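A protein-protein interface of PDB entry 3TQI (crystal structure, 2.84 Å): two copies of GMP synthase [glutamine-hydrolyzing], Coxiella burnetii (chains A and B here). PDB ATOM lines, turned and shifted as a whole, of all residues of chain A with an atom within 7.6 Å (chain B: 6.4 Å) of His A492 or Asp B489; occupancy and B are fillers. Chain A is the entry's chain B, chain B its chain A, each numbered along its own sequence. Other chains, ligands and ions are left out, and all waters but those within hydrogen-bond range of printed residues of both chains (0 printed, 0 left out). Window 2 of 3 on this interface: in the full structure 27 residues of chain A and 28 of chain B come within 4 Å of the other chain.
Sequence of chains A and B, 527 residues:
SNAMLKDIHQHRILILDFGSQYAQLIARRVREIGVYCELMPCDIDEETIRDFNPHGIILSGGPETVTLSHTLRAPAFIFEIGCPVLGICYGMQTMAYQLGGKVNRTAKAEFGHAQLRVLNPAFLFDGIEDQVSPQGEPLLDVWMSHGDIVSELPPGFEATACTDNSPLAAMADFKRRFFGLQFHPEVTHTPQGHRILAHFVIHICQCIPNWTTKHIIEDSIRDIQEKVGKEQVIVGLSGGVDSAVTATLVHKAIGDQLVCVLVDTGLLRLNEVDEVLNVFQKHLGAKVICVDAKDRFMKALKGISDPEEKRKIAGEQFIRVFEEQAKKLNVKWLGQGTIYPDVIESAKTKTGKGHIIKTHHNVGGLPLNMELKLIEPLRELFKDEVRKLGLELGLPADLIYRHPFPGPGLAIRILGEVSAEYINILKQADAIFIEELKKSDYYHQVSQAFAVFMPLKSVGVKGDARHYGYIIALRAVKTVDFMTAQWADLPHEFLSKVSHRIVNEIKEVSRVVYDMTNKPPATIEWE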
ATOM      1  N   ASP A 489     -13.750  -8.309 -20.625  1.00  0.00           N
ATOM      2  CA  ASP A 489     -13.707  -9.479 -21.502  1.00  0.00           C
ATOM      3  C   ASP A 489     -14.287 -10.681 -20.755  1.00  0.00           C
ATOM      4  O   ASP A 489     -13.572 -11.612 -20.414  1.00  0.00           O
ATOM      5  CB  ASP A 489     -12.250  -9.742 -21.940  1.00  0.00           C
ATOM      6  CG  ASP A 489     -12.107 -10.905 -22.933  1.00  0.00           C
ATOM      7  OD1 ASP A 489     -13.128 -11.409 -23.450  1.00  0.00           O
ATOM      8  OD2 ASP A 489     -10.953 -11.309 -23.201  1.00  0.00           O
ATOM      9  N   LEU A 490     -15.590 -10.653 -20.505  1.00  0.00           N
ATOM     10  CA  LEU A 490     -16.266 -11.753 -19.822  1.00  0.00           C
ATOM     11  C   LEU A 490     -16.639 -12.841 -20.827  1.00  0.00           C
ATOM     12  O   LEU A 490     -16.833 -12.548 -22.008  1.00  0.00           O
ATOM     13  CB  LEU A 490     -17.515 -11.250 -19.099  1.00  0.00           C
ATOM     14  CG  LEU A 490     -17.229 -10.268 -17.959  1.00  0.00           C
ATOM     15  CD1 LEU A 490     -18.509  -9.594 -17.500  1.00  0.00           C
ATOM     16  CD2 LEU A 490     -16.538 -10.963 -16.792  1.00  0.00           C
ATOM     17  N   PRO A 491     -16.747 -14.102 -20.364  1.00  0.00           N
ATOM     18  CA  PRO A 491     -16.942 -15.225 -21.281  1.00  0.00           C
ATOM     19  C   PRO A 491     -18.308 -15.272 -21.963  1.00  0.00           C
ATOM     20  O   PRO A 491     -19.317 -14.907 -21.366  1.00  0.00           O
ATOM     21  CB  PRO A 491     -16.769 -16.459 -20.378  1.00  0.00           C
ATOM     22  CG  PRO A 491     -16.218 -15.964 -19.107  1.00  0.00           C
ATOM     23  CD  PRO A 491     -16.680 -14.559 -18.968  1.00  0.00           C
ATOM     24  N   HIS A 492     -18.317 -15.748 -23.205  1.00  0.00           N
ATOM     25  CA  HIS A 492     -19.534 -15.848 -24.017  1.00  0.00           C
ATOM     26  C   HIS A 492     -20.637 -16.608 -23.280  1.00  0.00           C
ATOM     27  O   HIS A 492     -21.788 -16.169 -23.246  1.00  0.00           O
ATOM     28  CB  HIS A 492     -19.216 -16.550 -25.352  1.00  0.00           C
ATOM     29  CG  HIS A 492     -20.362 -16.565 -26.318  1.00  0.00           C
ATOM     30  ND1 HIS A 492     -21.309 -17.588 -26.364  1.00  0.00           N
ATOM     31  CD2 HIS A 492     -20.713 -15.681 -27.282  1.00  0.00           C
ATOM     32  CE1 HIS A 492     -22.197 -17.330 -27.311  1.00  0.00           C
ATOM     33  NE2 HIS A 492     -21.861 -16.173 -27.879  1.00  0.00           N
ATOM     34  N   GLU A 493     -20.263 -17.748 -22.699  1.00  0.00           N
ATOM     35  CA  GLU A 493     -21.174 -18.593 -21.926  1.00  0.00           C
ATOM     36  C   GLU A 493     -21.906 -17.800 -20.835  1.00  0.00           C
ATOM     37  O   GLU A 493     -23.124 -17.909 -20.686  1.00  0.00           O
ATOM     38  CB  GLU A 493     -20.366 -19.754 -21.330  1.00  0.00           C
ATOM     39  CG  GLU A 493     -21.116 -20.708 -20.423  1.00  0.00           C
ATOM     40  CD  GLU A 493     -20.292 -21.953 -20.089  1.00  0.00           C
ATOM     41  OE1 GLU A 493     -19.444 -21.878 -19.174  1.00  0.00           O
ATOM     42  OE2 GLU A 493     -20.488 -23.009 -20.731  1.00  0.00           O
ATOM     43  N   PHE A 494     -21.151 -16.982 -20.105  1.00  0.00           N
ATOM     44  CA  PHE A 494     -21.667 -16.209 -18.968  1.00  0.00           C
ATOM     45  C   PHE A 494     -22.559 -15.030 -19.369  1.00  0.00           C
ATOM     46  O   PHE A 494     -23.598 -14.791 -18.748  1.00  0.00           O
ATOM     47  CB  PHE A 494     -20.496 -15.694 -18.126  1.00  0.00           C
ATOM     48  CG  PHE A 494     -20.884 -14.661 -17.115  1.00  0.00           C
ATOM     49  CD1 PHE A 494     -21.276 -15.035 -15.844  1.00  0.00           C
ATOM     50  CD2 PHE A 494     -20.852 -13.308 -17.434  1.00  0.00           C
ATOM     51  CE1 PHE A 494     -21.632 -14.081 -14.904  1.00  0.00           C
ATOM     52  CE2 PHE A 494     -21.212 -12.346 -16.498  1.00  0.00           C
ATOM     53  CZ  PHE A 494     -21.603 -12.736 -15.232  1.00  0.00           C
ATOM     54  N   LEU A 495     -22.130 -14.273 -20.376  1.00  0.00           N
ATOM     55  CA  LEU A 495     -22.930 -13.154 -20.879  1.00  0.00           C
ATOM     56  C   LEU A 495     -24.260 -13.659 -21.415  1.00  0.00           C
ATOM     57  O   LEU A 495     -25.309 -13.080 -21.131  1.00  0.00           O
ATOM     58  CB  LEU A 495     -22.208 -12.389 -21.998  1.00  0.00           C
ATOM     59  CG  LEU A 495     -21.160 -11.317 -21.669  1.00  0.00           C
ATOM     60  CD1 LEU A 495     -21.340 -10.728 -20.264  1.00  0.00           C
ATOM     61  CD2 LEU A 495     -19.762 -11.878 -21.840  1.00  0.00           C
ATOM     62  N   SER A 496     -24.204 -14.733 -22.198  1.00  0.00           N
ATOM     63  CA  SER A 496     -25.406 -15.350 -22.727  1.00  0.00           C
ATOM     64  C   SER A 496     -26.365 -15.699 -21.603  1.00  0.00           C
ATOM     65  O   SER A 496     -27.561 -15.450 -21.720  1.00  0.00           O
ATOM     66  CB  SER A 496     -25.067 -16.596 -23.539  1.00  0.00           C
ATOM     67  OG  SER A 496     -24.340 -16.253 -24.706  1.00  0.00           O
ATOM     68  N   LYS A 497     -25.848 -16.251 -20.506  1.00  0.00           N
ATOM     69  CA  LYS A 497     -26.704 -16.590 -19.368  1.00  0.00           C
ATOM     70  C   LYS A 497     -27.390 -15.342 -18.839  1.00  0.00           C
ATOM     71  O   LYS A 497     -28.607 -15.322 -18.686  1.00  0.00           O
ATOM     72  CB  LYS A 497     -25.934 -17.285 -18.235  1.00  0.00           C
ATOM     73  CG  LYS A 497     -26.869 -17.965 -17.218  1.00  0.00           C
ATOM     74  CD  LYS A 497     -26.160 -18.956 -16.281  1.00  0.00           C
ATOM     75  CE  LYS A 497     -26.124 -18.464 -14.836  1.00  0.00           C
ATOM     76  NZ  LYS A 497     -25.720 -19.541 -13.877  1.00  0.00           N
ATOM     77  N   VAL A 498     -26.615 -14.296 -18.583  1.00  0.00           N
ATOM     78  CA  VAL A 498     -27.183 -13.064 -18.060  1.00  0.00           C
ATOM     79  C   VAL A 498     -28.286 -12.564 -18.979  1.00  0.00           C
ATOM     80  O   VAL A 498     -29.425 -12.399 -18.545  1.00  0.00           O
ATOM     81  CB  VAL A 498     -26.114 -11.972 -17.855  1.00  0.00           C
ATOM     82  CG1 VAL A 498     -26.764 -10.626 -17.592  1.00  0.00           C
ATOM     83  CG2 VAL A 498     -25.196 -12.349 -16.696  1.00  0.00           C
ATOM     84  N   SER A 499     -27.949 -12.359 -20.250  1.00  0.00           N
ATOM     85  CA  SER A 499     -28.876 -11.751 -21.218  1.00  0.00           C
ATOM     86  C   SER A 499     -30.171 -12.548 -21.405  1.00  0.00           C
ATOM     87  O   SER A 499     -31.260 -11.967 -21.414  1.00  0.00           O
ATOM     88  CB  SER A 499     -28.192 -11.564 -22.570  1.00  0.00           C
ATOM     89  OG  SER A 499     -27.895 -12.814 -23.156  1.00  0.00           O
ATOM     90  N   ALA B 476     -24.259  -9.517 -34.954  1.00  0.00           N
ATOM     91  CA  ALA B 476     -23.664 -10.594 -35.734  1.00  0.00           C
ATOM     92  C   ALA B 476     -24.067 -11.923 -35.137  1.00  0.00           C
ATOM     93  O   ALA B 476     -23.911 -12.130 -33.936  1.00  0.00           O
ATOM     94  CB  ALA B 476     -22.162 -10.465 -35.761  1.00  0.00           C
ATOM     95  N   GLN B 486     -28.139 -17.154 -31.393  1.00  0.00           N
ATOM     96  CA  GLN B 486     -26.786 -17.648 -31.577  1.00  0.00           C
ATOM     97  C   GLN B 486     -25.836 -16.508 -31.959  1.00  0.00           C
ATOM     98  O   GLN B 486     -25.208 -16.530 -33.012  1.00  0.00           O
ATOM     99  CB  GLN B 486     -26.778 -18.776 -32.617  1.00  0.00           C
ATOM    100  CG  GLN B 486     -27.398 -18.431 -33.992  1.00  0.00           C
ATOM    101  CD  GLN B 486     -28.883 -18.131 -33.941  1.00  0.00           C
ATOM    102  OE1 GLN B 486     -29.337 -17.327 -33.136  1.00  0.00           O
ATOM    103  NE2 GLN B 486     -29.646 -18.779 -34.814  1.00  0.00           N
ATOM    104  N   TRP B 487     -25.735 -15.510 -31.084  1.00  0.00           N
ATOM    105  CA  TRP B 487     -24.874 -14.353 -31.342  1.00  0.00           C
ATOM    106  C   TRP B 487     -23.422 -14.787 -31.369  1.00  0.00           C
ATOM    107  O   TRP B 487     -23.017 -15.644 -30.595  1.00  0.00           O
ATOM    108  CB  TRP B 487     -25.097 -13.215 -30.325  1.00  0.00           C
ATOM    109  CG  TRP B 487     -24.840 -13.553 -28.877  1.00  0.00           C
ATOM    110  CD1 TRP B 487     -25.684 -14.199 -28.023  1.00  0.00           C
ATOM    111  CD2 TRP B 487     -23.674 -13.229 -28.106  1.00  0.00           C
ATOM    112  NE1 TRP B 487     -25.112 -14.316 -26.777  1.00  0.00           N
ATOM    113  CE2 TRP B 487     -23.877 -13.725 -26.799  1.00  0.00           C
ATOM    114  CE3 TRP B 487     -22.475 -12.569 -28.395  1.00  0.00           C
ATOM    115  CZ2 TRP B 487     -22.928 -13.581 -25.781  1.00  0.00           C
ATOM    116  CZ3 TRP B 487     -21.529 -12.427 -27.379  1.00  0.00           C
ATOM    117  CH2 TRP B 487     -21.763 -12.932 -26.089  1.00  0.00           C
ATOM    118  N   ALA B 488     -22.650 -14.191 -32.270  1.00  0.00           N
ATOM    119  CA  ALA B 488     -21.307 -14.675 -32.589  1.00  0.00           C
ATOM    120  C   ALA B 488     -20.279 -14.322 -31.517  1.00  0.00           C
ATOM    121  O   ALA B 488     -20.243 -13.194 -31.025  1.00  0.00           O
ATOM    122  CB  ALA B 488     -20.868 -14.132 -33.939  1.00  0.00           C
ATOM    123  N   ASP B 489     -19.437 -15.294 -31.181  1.00  0.00           N
ATOM    124  CA  ASP B 489     -18.459 -15.153 -30.110  1.00  0.00           C
ATOM    125  C   ASP B 489     -17.155 -14.634 -30.705  1.00  0.00           C
ATOM    126  O   ASP B 489     -16.154 -15.339 -30.733  1.00  0.00           O
ATOM    127  CB  ASP B 489     -18.272 -16.516 -29.409  1.00  0.00           C
ATOM    128  CG  ASP B 489     -17.237 -16.488 -28.282  1.00  0.00           C
ATOM    129  OD1 ASP B 489     -16.956 -15.413 -27.708  1.00  0.00           O
ATOM    130  OD2 ASP B 489     -16.704 -17.571 -27.965  1.00  0.00           O
ATOM    131  N   LEU B 490     -17.171 -13.397 -31.187  1.00  0.00           N
ATOM    132  CA  LEU B 490     -15.982 -12.789 -31.781  1.00  0.00           C
ATOM    133  C   LEU B 490     -14.965 -12.405 -30.700  1.00  0.00           C
ATOM    134  O   LEU B 490     -15.345 -12.161 -29.549  1.00  0.00           O
ATOM    135  CB  LEU B 490     -16.370 -11.561 -32.595  1.00  0.00           C
ATOM    136  CG  LEU B 490     -17.199 -11.853 -33.851  1.00  0.00           C
ATOM    137  CD1 LEU B 490     -18.030 -10.647 -34.230  1.00  0.00           C
ATOM    138  CD2 LEU B 490     -16.303 -12.283 -35.013  1.00  0.00           C
ATOM    139  N   PRO B 491     -13.666 -12.347 -31.060  1.00  0.00           N
ATOM    140  CA  PRO B 491     -12.638 -12.150 -30.046  1.00  0.00           C
ATOM    141  C   PRO B 491     -12.578 -10.725 -29.529  1.00  0.00           C
ATOM    142  O   PRO B 491     -12.662  -9.778 -30.307  1.00  0.00           O
ATOM    143  CB  PRO B 491     -11.332 -12.497 -30.776  1.00  0.00           C
ATOM    144  CG  PRO B 491     -11.708 -12.912 -32.148  1.00  0.00           C
ATOM    145  CD  PRO B 491     -13.082 -12.416 -32.407  1.00  0.00           C
ATOM    146  N   LEU B 495     -13.160  -7.036 -31.524  1.00  0.00           N
ATOM    147  CA  LEU B 495     -14.301  -6.163 -31.248  1.00  0.00           C
ATOM    148  C   LEU B 495     -13.827  -4.784 -30.839  1.00  0.00           C
ATOM    149  O   LEU B 495     -14.357  -3.782 -31.315  1.00  0.00           O
ATOM    150  CB  LEU B 495     -15.193  -6.715 -30.132  1.00  0.00           C
ATOM    151  CG  LEU B 495     -16.223  -7.797 -30.458  1.00  0.00           C
ATOM    152  CD1 LEU B 495     -16.811  -7.635 -31.862  1.00  0.00           C
ATOM    153  CD2 LEU B 495     -15.595  -9.162 -30.287  1.00  0.00           C
ATOM    154  N   TYR B 514     -22.926  -4.152 -28.521  1.00  0.00           N
ATOM    155  CA  TYR B 514     -22.976  -5.426 -29.221  1.00  0.00           C
ATOM    156  C   TYR B 514     -24.157  -6.223 -28.707  1.00  0.00           C
ATOM    157  O   TYR B 514     -24.292  -6.437 -27.499  1.00  0.00           O
ATOM    158  CB  TYR B 514     -21.679  -6.187 -28.955  1.00  0.00           C
ATOM    159  CG  TYR B 514     -21.458  -7.444 -29.779  1.00  0.00           C
ATOM    160  CD1 TYR B 514     -21.494  -7.409 -31.154  1.00  0.00           C
ATOM    161  CD2 TYR B 514     -21.156  -8.655 -29.170  1.00  0.00           C
ATOM    162  CE1 TYR B 514     -21.272  -8.551 -31.901  1.00  0.00           C
ATOM    163  CE2 TYR B 514     -20.933  -9.798 -29.909  1.00  0.00           C
ATOM    164  CZ  TYR B 514     -20.992  -9.742 -31.273  1.00  0.00           C
ATOM    165  OH  TYR B 514     -20.767 -10.877 -32.022  1.00  0.00           O
ATOM    166  N   ASN B 518     -30.241 -14.107 -28.519  1.00  0.00           N
ATOM    167  CA  ASN B 518     -30.277 -15.237 -29.457  1.00  0.00           C
ATOM    168  C   ASN B 518     -31.502 -15.289 -30.371  1.00  0.00           C
ATOM    169  O   ASN B 518     -32.462 -14.548 -30.183  1.00  0.00           O
ATOM    170  CB  ASN B 518     -30.175 -16.568 -28.693  1.00  0.00           C
ATOM    171  CG  ASN B 518     -28.763 -16.886 -28.232  1.00  0.00           C
ATOM    172  OD1 ASN B 518     -27.782 -16.427 -28.807  1.00  0.00           O
ATOM    173  ND2 ASN B 518     -28.661 -17.702 -27.196  1.00  0.00           N
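NE1 of Trp B487 sits at hydrogen-bond distance from OG of Ser A496, 2.9 Å away. O of Trp B487 sits at hydrogen-bond distance from NE2 of His A492 (3.0 Å).
N of Trp B487 lies close to OD1 of Asn B518 (3.2 Å). The side-chain hydroxyl (OG) of Ser A499 is in hydrogen-bond range of the backbone carbonyl oxygen (O) of Ser A496 (3.0 Å). O of His A492 is in hydrogen-bond range of OG of Ser A496 (2.9 Å).
CD2 of His A492 touches CB of Asp B489, at 3.3 Å.
Printed residues of chain A within 4 Å of Trp B487: His A492 (3.0 Å) and Ser A496 (2.9 Å). Printed residues of chain B within 4 Å of Ser A496: Trp B487. The nearest residue of chain B that does not touch His A492 is Ala B488 (4.4 Å). The nearest printed residue of chain B that does not touch Ser A496 is Asn B518 (5.2 Å).
Hydrophobic or aromatic side chains of chain A that line the printed part of chain B: His A492. Among the printed residues, no Asp or Glu carboxylate lies within 4 Å of a Lys or Arg side-chain nitrogen of the other chain.
4 positions are printed for both chains. Of the 3 pairs that touch across the chains among the printed residues, none has its exchanged pair printed and touching as well.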
